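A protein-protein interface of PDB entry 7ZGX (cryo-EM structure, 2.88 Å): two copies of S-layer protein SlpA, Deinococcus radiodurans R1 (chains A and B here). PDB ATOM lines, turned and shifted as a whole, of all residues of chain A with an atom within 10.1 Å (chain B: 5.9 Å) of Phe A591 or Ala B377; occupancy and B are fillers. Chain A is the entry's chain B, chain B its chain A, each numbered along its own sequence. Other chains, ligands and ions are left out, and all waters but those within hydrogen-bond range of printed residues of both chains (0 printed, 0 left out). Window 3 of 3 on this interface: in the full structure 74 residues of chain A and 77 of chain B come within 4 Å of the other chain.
The backbone carbonyl oxygen (O) of Gly A587 lies within hydrogen-bond range of the backbone NH (N) of Tyr A563 (2.9 Å). The backbone carbonyl oxygen (O) of Arg B378 lies within hydrogen-bond range of the backbone NH (N) of Thr B269, at 3.2 Å. The backbone NH of Gly A592 sits at hydrogen-bond distance from the side-chain carboxylate of Asp A589 (3.2 Å). OG1 of Thr B269 lies within hydrogen-bond range of N of Arg B271 (3.3 Å). N of Asp A589 sits at hydrogen-bond distance from O of Gly A561, 3.2 Å away. The side-chain hydroxyl (OH) of Tyr A560 sits at hydrogen-bond distance from the side-chain amide oxygen (OE1) of Gln A595.
No position is printed for both chains. Of the 12 pairs that touch across the chains among the printed residues, none has its exchanged pair printed and touching as well.
CD2 of Tyr B379 touches OH of Tyr A560, 3.7 Å away. Tyr B379 touches Gly A561. Tyr A563 touches Arg B268. Met A590 touches Arg B268. Met A590 touches Thr B269 (CE to O, 3.6 Å). Phe A591 touches Thr B269. CZ of Phe A591 touches CB of Ala B377, at 3.5 Å. Phe A591 touches Arg B378 (CZ to O, 3.5 Å). Tyr B379 touches Phe A591 (CD1 to CD2, 3.4 Å).
Phe A591 touches just these residues of chain B: Thr B269, Ala B377, Arg B378 and Tyr B379. No residue of chain A comes within 4 Å of Asn B375. Arg B378 touches just one residue of chain A: Phe A591. Printed residues of chain A within 4 Å of Arg B268: Tyr A563 (3.5 Å), Asp A589 (2.9 Å) and Met A590 (3.6 Å). Of the printed residues of chain B, Met A590 touches Arg B268 (3.6 Å) and Thr B269 (3.6 Å). Of the printed residues of chain A, Thr B269 touches Met A590 (3.6 Å) and Phe A591 (3.2 Å). Printed residues of chain B within 4 Å of Tyr A560: Tyr B379 (3.7 Å). Of the printed residues of chain B, Gly A561 touches Tyr B379 (3.6 Å). The nearest residue of chain B that does not touch Phe A591 is Arg B268 (4.05 Å). The nearest residue of chain A that does not touch Ala B377 is Met A590 (6.6 Å).
The side-chain hydroxyl of Tyr B379 sits at hydrogen-bond distance from the side-chain carboxylate of Asp A589, at 3.0 Å. NE of Arg B268 lies within salt-bridge range of OD2 of Asp A589 (2.9 Å). The side-chain hydroxyl of Tyr A563 sits close to the side-chain hydroxyl of Tyr B379 (2.3 Å).
Of the 23 printed residues of chain A, 6 touch a printed residue of chain B. Of the 10 printed residues of chain B, 5 touch a printed residue of chain A. Among the printed residues, Asp or Glu carboxylates within 4 Å of a Lys or Arg side-chain nitrogen of the other chain: Asp A589 with Arg B268.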
ATOM      1  N   ASP A 553      -9.908  10.057 -19.957  1.00  0.00           N
ATOM      2  CA  ASP A 553      -8.497   9.798 -19.745  1.00  0.00           C
ATOM      3  C   ASP A 553      -7.680  10.898 -20.401  1.00  0.00           C
ATOM      4  O   ASP A 553      -8.148  11.600 -21.298  1.00  0.00           O
ATOM      5  CB  ASP A 553      -8.106   8.416 -20.278  1.00  0.00           C
ATOM      6  CG  ASP A 553      -8.453   8.236 -21.735  1.00  0.00           C
ATOM      7  OD1 ASP A 553      -9.057   9.153 -22.324  1.00  0.00           O
ATOM      8  OD2 ASP A 553      -8.135   7.168 -22.291  1.00  0.00           O
ATOM      9  N   GLY A 554      -6.443  11.048 -19.937  1.00  0.00           N
ATOM     10  CA  GLY A 554      -5.589  12.122 -20.387  1.00  0.00           C
ATOM     11  C   GLY A 554      -5.132  11.940 -21.819  1.00  0.00           C
ATOM     12  O   GLY A 554      -5.297  10.887 -22.434  1.00  0.00           O
ATOM     13  N   THR A 555      -4.551  13.006 -22.355  1.00  0.00           N
ATOM     14  CA  THR A 555      -4.007  12.967 -23.700  1.00  0.00           C
ATOM     15  C   THR A 555      -2.821  12.007 -23.740  1.00  0.00           C
ATOM     16  O   THR A 555      -2.241  11.656 -22.710  1.00  0.00           O
ATOM     17  CB  THR A 555      -3.592  14.371 -24.138  1.00  0.00           C
ATOM     18  OG1 THR A 555      -4.682  15.269 -23.917  1.00  0.00           O
ATOM     19  CG2 THR A 555      -3.257  14.407 -25.615  1.00  0.00           C
ATOM     20  N   ALA A 556      -2.485  11.555 -24.947  1.00  0.00           N
ATOM     21  CA  ALA A 556      -1.409  10.611 -25.226  1.00  0.00           C
ATOM     22  C   ALA A 556      -1.716   9.209 -24.728  1.00  0.00           C
ATOM     23  O   ALA A 556      -0.826   8.353 -24.724  1.00  0.00           O
ATOM     24  CB  ALA A 556      -0.065  11.073 -24.654  1.00  0.00           C
ATOM     25  N   GLU A 557      -2.946   8.949 -24.302  1.00  0.00           N
ATOM     26  CA  GLU A 557      -3.425   7.598 -24.065  1.00  0.00           C
ATOM     27  C   GLU A 557      -4.298   7.163 -25.231  1.00  0.00           C
ATOM     28  O   GLU A 557      -4.916   7.983 -25.912  1.00  0.00           O
ATOM     29  CB  GLU A 557      -4.207   7.501 -22.754  1.00  0.00           C
ATOM     30  CG  GLU A 557      -3.360   7.696 -21.514  1.00  0.00           C
ATOM     31  CD  GLU A 557      -4.049   7.206 -20.260  1.00  0.00           C
ATOM     32  OE1 GLU A 557      -4.629   6.103 -20.294  1.00  0.00           O
ATOM     33  OE2 GLU A 557      -4.011   7.922 -19.239  1.00  0.00           O
ATOM     34  N   GLY A 559      -7.099   5.967 -25.459  1.00  0.00           N
ATOM     35  CA  GLY A 559      -8.535   6.126 -25.361  1.00  0.00           C
ATOM     36  C   GLY A 559      -9.018   7.553 -25.209  1.00  0.00           C
ATOM     37  O   GLY A 559     -10.041   7.794 -24.563  1.00  0.00           O
ATOM     38  N   TYR A 560      -8.303   8.506 -25.798  1.00  0.00           N
ATOM     39  CA  TYR A 560      -8.695   9.911 -25.724  1.00  0.00           C
ATOM     40  C   TYR A 560      -9.534  10.254 -26.944  1.00  0.00           C
ATOM     41  O   TYR A 560      -9.070  10.160 -28.080  1.00  0.00           O
ATOM     42  CB  TYR A 560      -7.478  10.820 -25.637  1.00  0.00           C
ATOM     43  CG  TYR A 560      -7.850  12.262 -25.404  1.00  0.00           C
ATOM     44  CD1 TYR A 560      -8.274  12.694 -24.162  1.00  0.00           C
ATOM     45  CD2 TYR A 560      -7.803  13.186 -26.433  1.00  0.00           C
ATOM     46  CE1 TYR A 560      -8.625  14.007 -23.945  1.00  0.00           C
ATOM     47  CE2 TYR A 560      -8.154  14.502 -26.225  1.00  0.00           C
ATOM     48  CZ  TYR A 560      -8.564  14.904 -24.979  1.00  0.00           C
ATOM     49  OH  TYR A 560      -8.914  16.213 -24.761  1.00  0.00           O
ATOM     50  N   GLY A 561     -10.775  10.661 -26.708  1.00  0.00           N
ATOM     51  CA  GLY A 561     -11.634  11.084 -27.792  1.00  0.00           C
ATOM     52  C   GLY A 561     -11.960  10.008 -28.795  1.00  0.00           C
ATOM     53  O   GLY A 561     -12.101  10.304 -29.983  1.00  0.00           O
ATOM     54  N   VAL A 562     -12.081   8.761 -28.356  1.00  0.00           N
ATOM     55  CA  VAL A 562     -12.459   7.655 -29.224  1.00  0.00           C
ATOM     56  C   VAL A 562     -13.742   7.040 -28.691  1.00  0.00           C
ATOM     57  O   VAL A 562     -13.845   6.715 -27.500  1.00  0.00           O
ATOM     58  CB  VAL A 562     -11.339   6.611 -29.340  1.00  0.00           C
ATOM     59  CG1 VAL A 562     -10.213   7.153 -30.176  1.00  0.00           C
ATOM     60  CG2 VAL A 562     -10.809   6.287 -27.996  1.00  0.00           C
ATOM     61  N   TYR A 563     -14.720   6.893 -29.575  1.00  0.00           N
ATOM     62  CA  TYR A 563     -16.039   6.400 -29.223  1.00  0.00           C
ATOM     63  C   TYR A 563     -16.398   5.241 -30.133  1.00  0.00           C
ATOM     64  O   TYR A 563     -16.052   5.232 -31.317  1.00  0.00           O
ATOM     65  CB  TYR A 563     -17.086   7.505 -29.333  1.00  0.00           C
ATOM     66  CG  TYR A 563     -16.792   8.685 -28.448  1.00  0.00           C
ATOM     67  CD1 TYR A 563     -15.938   9.687 -28.862  1.00  0.00           C
ATOM     68  CD2 TYR A 563     -17.358   8.792 -27.195  1.00  0.00           C
ATOM     69  CE1 TYR A 563     -15.660  10.763 -28.056  1.00  0.00           C
ATOM     70  CE2 TYR A 563     -17.085   9.864 -26.383  1.00  0.00           C
ATOM     71  CZ  TYR A 563     -16.235  10.846 -26.818  1.00  0.00           C
ATOM     72  OH  TYR A 563     -15.960  11.919 -26.008  1.00  0.00           O
ATOM     73  N   GLY A 587     -14.212   5.095 -33.604  1.00  0.00           N
ATOM     74  CA  GLY A 587     -13.545   6.196 -34.267  1.00  0.00           C
ATOM     75  C   GLY A 587     -13.192   7.343 -33.349  1.00  0.00           C
ATOM     76  O   GLY A 587     -13.418   7.306 -32.139  1.00  0.00           O
ATOM     77  N   ARG A 588     -12.616   8.374 -33.963  1.00  0.00           N
ATOM     78  CA  ARG A 588     -12.213   9.592 -33.279  1.00  0.00           C
ATOM     79  C   ARG A 588     -13.189  10.718 -33.581  1.00  0.00           C
ATOM     80  O   ARG A 588     -13.679  10.844 -34.705  1.00  0.00           O
ATOM     81  CB  ARG A 588     -10.815  10.013 -33.724  1.00  0.00           C
ATOM     82  CG  ARG A 588      -9.686   9.301 -33.041  1.00  0.00           C
ATOM     83  CD  ARG A 588      -8.387  10.006 -33.343  1.00  0.00           C
ATOM     84  NE  ARG A 588      -7.270   9.086 -33.494  1.00  0.00           N
ATOM     85  CZ  ARG A 588      -6.000   9.443 -33.386  1.00  0.00           C
ATOM     86  NH1 ARG A 588      -5.653  10.695 -33.148  1.00  0.00           N
ATOM     87  NH2 ARG A 588      -5.053   8.520 -33.515  1.00  0.00           N
ATOM     88  N   ASP A 589     -13.460  11.544 -32.577  1.00  0.00           N
ATOM     89  CA  ASP A 589     -14.289  12.724 -32.766  1.00  0.00           C
ATOM     90  C   ASP A 589     -13.383  13.930 -33.014  1.00  0.00           C
ATOM     91  O   ASP A 589     -12.164  13.785 -33.143  1.00  0.00           O
ATOM     92  CB  ASP A 589     -15.217  12.904 -31.567  1.00  0.00           C
ATOM     93  CG  ASP A 589     -14.468  13.200 -30.302  1.00  0.00           C
ATOM     94  OD1 ASP A 589     -13.269  12.871 -30.240  1.00  0.00           O
ATOM     95  OD2 ASP A 589     -15.074  13.761 -29.368  1.00  0.00           O
ATOM     96  N   MET A 590     -13.954  15.136 -33.073  1.00  0.00           N
ATOM     97  CA  MET A 590     -13.176  16.300 -33.481  1.00  0.00           C
ATOM     98  C   MET A 590     -12.121  16.686 -32.455  1.00  0.00           C
ATOM     99  O   MET A 590     -11.161  17.382 -32.799  1.00  0.00           O
ATOM    100  CB  MET A 590     -14.094  17.491 -33.752  1.00  0.00           C
ATOM    101  CG  MET A 590     -14.830  18.022 -32.539  1.00  0.00           C
ATOM    102  SD  MET A 590     -15.913  19.388 -32.999  1.00  0.00           S
ATOM    103  CE  MET A 590     -16.652  19.803 -31.427  1.00  0.00           C
ATOM    104  N   PHE A 591     -12.275  16.258 -31.208  1.00  0.00           N
ATOM    105  CA  PHE A 591     -11.265  16.474 -30.181  1.00  0.00           C
ATOM    106  C   PHE A 591     -10.276  15.326 -30.088  1.00  0.00           C
ATOM    107  O   PHE A 591      -9.373  15.367 -29.247  1.00  0.00           O
ATOM    108  CB  PHE A 591     -11.931  16.689 -28.827  1.00  0.00           C
ATOM    109  CG  PHE A 591     -12.451  18.067 -28.636  1.00  0.00           C
ATOM    110  CD1 PHE A 591     -11.616  19.078 -28.223  1.00  0.00           C
ATOM    111  CD2 PHE A 591     -13.772  18.360 -28.895  1.00  0.00           C
ATOM    112  CE1 PHE A 591     -12.093  20.348 -28.057  1.00  0.00           C
ATOM    113  CE2 PHE A 591     -14.252  19.629 -28.731  1.00  0.00           C
ATOM    114  CZ  PHE A 591     -13.415  20.624 -28.311  1.00  0.00           C
ATOM    115  N   GLY A 592     -10.433  14.302 -30.915  1.00  0.00           N
ATOM    116  CA  GLY A 592      -9.493  13.207 -30.944  1.00  0.00           C
ATOM    117  C   GLY A 592      -8.638  13.259 -32.187  1.00  0.00           C
ATOM    118  O   GLY A 592      -7.481  12.840 -32.165  1.00  0.00           O
ATOM    119  N   ALA A 593      -9.197  13.774 -33.283  1.00  0.00           N
ATOM    120  CA  ALA A 593      -8.418  13.891 -34.511  1.00  0.00           C
ATOM    121  C   ALA A 593      -7.181  14.746 -34.286  1.00  0.00           C
ATOM    122  O   ALA A 593      -6.111  14.466 -34.839  1.00  0.00           O
ATOM    123  CB  ALA A 593      -9.282  14.468 -35.629  1.00  0.00           C
ATOM    124  N   ALA A 594      -7.310  15.786 -33.477  1.00  0.00           N
ATOM    125  CA  ALA A 594      -6.186  16.561 -32.984  1.00  0.00           C
ATOM    126  C   ALA A 594      -6.080  16.376 -31.479  1.00  0.00           C
ATOM    127  O   ALA A 594      -7.065  16.069 -30.803  1.00  0.00           O
ATOM    128  CB  ALA A 594      -6.345  18.045 -33.325  1.00  0.00           C
ATOM    129  N   GLN A 595      -4.862  16.541 -30.962  1.00  0.00           N
ATOM    130  CA  GLN A 595      -4.605  16.493 -29.524  1.00  0.00           C
ATOM    131  C   GLN A 595      -4.846  15.078 -28.983  1.00  0.00           C
ATOM    132  O   GLN A 595      -5.507  14.869 -27.966  1.00  0.00           O
ATOM    133  CB  GLN A 595      -5.454  17.548 -28.801  1.00  0.00           C
ATOM    134  CG  GLN A 595      -5.307  17.661 -27.294  1.00  0.00           C
ATOM    135  CD  GLN A 595      -6.473  18.395 -26.667  1.00  0.00           C
ATOM    136  OE1 GLN A 595      -6.950  18.028 -25.596  1.00  0.00           O
ATOM    137  NE2 GLN A 595      -6.947  19.435 -27.343  1.00  0.00           N
ATOM    138  N   ASN A 596      -4.313  14.088 -29.698  1.00  0.00           N
ATOM    139  CA  ASN A 596      -4.397  12.698 -29.254  1.00  0.00           C
ATOM    140  C   ASN A 596      -3.087  11.935 -29.319  1.00  0.00           C
ATOM    141  O   ASN A 596      -2.901  11.016 -28.515  1.00  0.00           O
ATOM    142  CB  ASN A 596      -5.439  11.934 -30.076  1.00  0.00           C
ATOM    143  CG  ASN A 596      -5.636  10.510 -29.596  1.00  0.00           C
ATOM    144  OD1 ASN A 596      -5.972   9.623 -30.377  1.00  0.00           O
ATOM    145  ND2 ASN A 596      -5.436  10.285 -28.307  1.00  0.00           N
ATOM    146  N   THR A 597      -2.166  12.281 -30.218  1.00  0.00           N
ATOM    147  CA  THR A 597      -0.964  11.496 -30.468  1.00  0.00           C
ATOM    148  C   THR A 597      -1.316  10.031 -30.697  1.00  0.00           C
ATOM    149  O   THR A 597      -2.206   9.722 -31.496  1.00  0.00           O
ATOM    150  CB  THR A 597       0.027  11.628 -29.310  1.00  0.00           C
ATOM    151  OG1 THR A 597      -0.395  10.791 -28.232  1.00  0.00           O
ATOM    152  CG2 THR A 597       0.095  13.063 -28.826  1.00  0.00           C
ATOM    153  N   THR A 598      -0.646   9.129 -29.977  1.00  0.00           N
ATOM    154  CA  THR A 598      -0.801   7.683 -30.127  1.00  0.00           C
ATOM    155  C   THR A 598      -0.830   7.247 -31.588  1.00  0.00           C
ATOM    156  O   THR A 598      -0.244   7.904 -32.454  1.00  0.00           O
ATOM    157  CB  THR A 598      -2.067   7.190 -29.425  1.00  0.00           C
ATOM    158  OG1 THR A 598      -3.177   8.016 -29.786  1.00  0.00           O
ATOM    159  CG2 THR A 598      -1.884   7.226 -27.924  1.00  0.00           C
ATOM    160  N   ASN A 632      -5.149   7.054 -39.464  1.00  0.00           N
ATOM    161  CA  ASN A 632      -4.677   8.374 -39.061  1.00  0.00           C
ATOM    162  C   ASN A 632      -3.863   9.065 -40.151  1.00  0.00           C
ATOM    163  O   ASN A 632      -4.352   9.255 -41.269  1.00  0.00           O
ATOM    164  CB  ASN A 632      -3.844   8.262 -37.783  1.00  0.00           C
ATOM    165  CG  ASN A 632      -4.110   9.392 -36.816  1.00  0.00           C
ATOM    166  OD1 ASN A 632      -5.072  10.139 -36.967  1.00  0.00           O
ATOM    167  ND2 ASN A 632      -3.252   9.524 -35.814  1.00  0.00           N
ATOM    168  N   SER B 267     -19.816  16.203 -23.963  1.00  0.00           N
ATOM    169  CA  SER B 267     -20.148  17.523 -24.475  1.00  0.00           C
ATOM    170  C   SER B 267     -18.982  18.058 -25.286  1.00  0.00           C
ATOM    171  O   SER B 267     -17.857  18.133 -24.791  1.00  0.00           O
ATOM    172  CB  SER B 267     -20.483  18.487 -23.339  1.00  0.00           C
ATOM    173  OG  SER B 267     -20.653  19.801 -23.831  1.00  0.00           O
ATOM    174  N   ARG B 268     -19.261  18.432 -26.532  1.00  0.00           N
ATOM    175  CA  ARG B 268     -18.239  18.952 -27.425  1.00  0.00           C
ATOM    176  C   ARG B 268     -18.708  20.272 -28.008  1.00  0.00           C
ATOM    177  O   ARG B 268     -19.791  20.343 -28.592  1.00  0.00           O
ATOM    178  CB  ARG B 268     -17.939  17.970 -28.560  1.00  0.00           C
ATOM    179  CG  ARG B 268     -18.015  16.514 -28.177  1.00  0.00           C
ATOM    180  CD  ARG B 268     -17.851  15.650 -29.406  1.00  0.00           C
ATOM    181  NE  ARG B 268     -17.883  14.228 -29.098  1.00  0.00           N
ATOM    182  CZ  ARG B 268     -18.991  13.534 -28.883  1.00  0.00           C
ATOM    183  NH1 ARG B 268     -20.180  14.108 -28.909  1.00  0.00           N
ATOM    184  NH2 ARG B 268     -18.904  12.232 -28.639  1.00  0.00           N
ATOM    185  N   THR B 269     -17.889  21.307 -27.872  1.00  0.00           N
ATOM    186  CA  THR B 269     -18.186  22.610 -28.442  1.00  0.00           C
ATOM    187  C   THR B 269     -16.937  23.184 -29.088  1.00  0.00           C
ATOM    188  O   THR B 269     -15.887  22.542 -29.147  1.00  0.00           O
ATOM    189  CB  THR B 269     -18.711  23.585 -27.389  1.00  0.00           C
ATOM    190  OG1 THR B 269     -19.065  24.817 -28.025  1.00  0.00           O
ATOM    191  CG2 THR B 269     -17.647  23.854 -26.358  1.00  0.00           C
ATOM    192  N   SER B 270     -17.066  24.409 -29.585  1.00  0.00           N
ATOM    193  CA  SER B 270     -15.936  25.139 -30.132  1.00  0.00           C
ATOM    194  C   SER B 270     -15.897  26.591 -29.685  1.00  0.00           C
ATOM    195  O   SER B 270     -14.867  27.248 -29.866  1.00  0.00           O
ATOM    196  CB  SER B 270     -15.947  25.070 -31.662  1.00  0.00           C
ATOM    197  OG  SER B 270     -17.016  25.825 -32.195  1.00  0.00           O
ATOM    198  N   ARG B 271     -16.979  27.112 -29.111  1.00  0.00           N
ATOM    199  CA  ARG B 271     -17.006  28.493 -28.653  1.00  0.00           C
ATOM    200  C   ARG B 271     -17.621  28.598 -27.262  1.00  0.00           C
ATOM    201  O   ARG B 271     -17.379  29.574 -26.547  1.00  0.00           O
ATOM    202  CB  ARG B 271     -17.779  29.358 -29.646  1.00  0.00           C
ATOM    203  CG  ARG B 271     -17.744  30.847 -29.375  1.00  0.00           C
ATOM    204  CD  ARG B 271     -16.365  31.426 -29.549  1.00  0.00           C
ATOM    205  NE  ARG B 271     -16.324  32.832 -29.174  1.00  0.00           N
ATOM    206  CZ  ARG B 271     -16.536  33.837 -30.010  1.00  0.00           C
ATOM    207  NH1 ARG B 271     -16.834  33.629 -31.281  1.00  0.00           N
ATOM    208  NH2 ARG B 271     -16.448  35.085 -29.560  1.00  0.00           N
ATOM    209  N   ASN B 375      -7.477  28.960 -26.378  1.00  0.00           N
ATOM    210  CA  ASN B 375      -8.328  28.121 -27.207  1.00  0.00           C
ATOM    211  C   ASN B 375      -9.773  28.226 -26.745  1.00  0.00           C
ATOM    212  O   ASN B 375     -10.064  28.164 -25.549  1.00  0.00           O
ATOM    213  CB  ASN B 375      -7.855  26.670 -27.144  1.00  0.00           C
ATOM    214  CG  ASN B 375      -8.346  25.851 -28.313  1.00  0.00           C
ATOM    215  OD1 ASN B 375      -8.562  26.376 -29.403  1.00  0.00           O
ATOM    216  ND2 ASN B 375      -8.523  24.555 -28.094  1.00  0.00           N
ATOM    217  N   LEU B 376     -10.680  28.400 -27.701  1.00  0.00           N
ATOM    218  CA  LEU B 376     -12.084  28.608 -27.390  1.00  0.00           C
ATOM    219  C   LEU B 376     -12.897  27.325 -27.381  1.00  0.00           C
ATOM    220  O   LEU B 376     -14.103  27.378 -27.129  1.00  0.00           O
ATOM    221  CB  LEU B 376     -12.704  29.592 -28.383  1.00  0.00           C
ATOM    222  CG  LEU B 376     -12.189  31.013 -28.209  1.00  0.00           C
ATOM    223  CD1 LEU B 376     -12.803  31.933 -29.239  1.00  0.00           C
ATOM    224  CD2 LEU B 376     -12.492  31.490 -26.806  1.00  0.00           C
ATOM    225  N   ALA B 377     -12.279  26.186 -27.653  1.00  0.00           N
ATOM    226  CA  ALA B 377     -12.993  24.922 -27.632  1.00  0.00           C
ATOM    227  C   ALA B 377     -12.982  24.336 -26.232  1.00  0.00           C
ATOM    228  O   ALA B 377     -11.955  24.337 -25.551  1.00  0.00           O
ATOM    229  CB  ALA B 377     -12.360  23.941 -28.615  1.00  0.00           C
ATOM    230  N   ARG B 378     -14.133  23.837 -25.800  1.00  0.00           N
ATOM    231  CA  ARG B 378     -14.251  23.127 -24.539  1.00  0.00           C
ATOM    232  C   ARG B 378     -14.748  21.716 -24.806  1.00  0.00           C
ATOM    233  O   ARG B 378     -15.557  21.488 -25.706  1.00  0.00           O
ATOM    234  CB  ARG B 378     -15.190  23.844 -23.571  1.00  0.00           C
ATOM    235  CG  ARG B 378     -14.531  24.986 -22.825  1.00  0.00           C
ATOM    236  CD  ARG B 378     -14.659  26.284 -23.587  1.00  0.00           C
ATOM    237  NE  ARG B 378     -14.109  27.413 -22.849  1.00  0.00           N
ATOM    238  CZ  ARG B 378     -12.908  27.928 -23.065  1.00  0.00           C
ATOM    239  NH1 ARG B 378     -12.113  27.454 -24.005  1.00  0.00           N
ATOM    240  NH2 ARG B 378     -12.500  28.952 -22.324  1.00  0.00           N
ATOM    241  N   TYR B 379     -14.253  20.766 -24.018  1.00  0.00           N
ATOM    242  CA  TYR B 379     -14.525  19.360 -24.266  1.00  0.00           C
ATOM    243  C   TYR B 379     -14.737  18.649 -22.941  1.00  0.00           C
ATOM    244  O   TYR B 379     -14.085  18.967 -21.946  1.00  0.00           O
ATOM    245  CB  TYR B 379     -13.373  18.711 -25.037  1.00  0.00           C
ATOM    246  CG  TYR B 379     -13.604  17.274 -25.438  1.00  0.00           C
ATOM    247  CD1 TYR B 379     -14.804  16.874 -25.994  1.00  0.00           C
ATOM    248  CD2 TYR B 379     -12.613  16.321 -25.273  1.00  0.00           C
ATOM    249  CE1 TYR B 379     -15.010  15.568 -26.368  1.00  0.00           C
ATOM    250  CE2 TYR B 379     -12.817  15.014 -25.644  1.00  0.00           C
ATOM    251  CZ  TYR B 379     -14.015  14.645 -26.190  1.00  0.00           C
ATOM    252  OH  TYR B 379     -14.223  13.341 -26.560  1.00  0.00           O
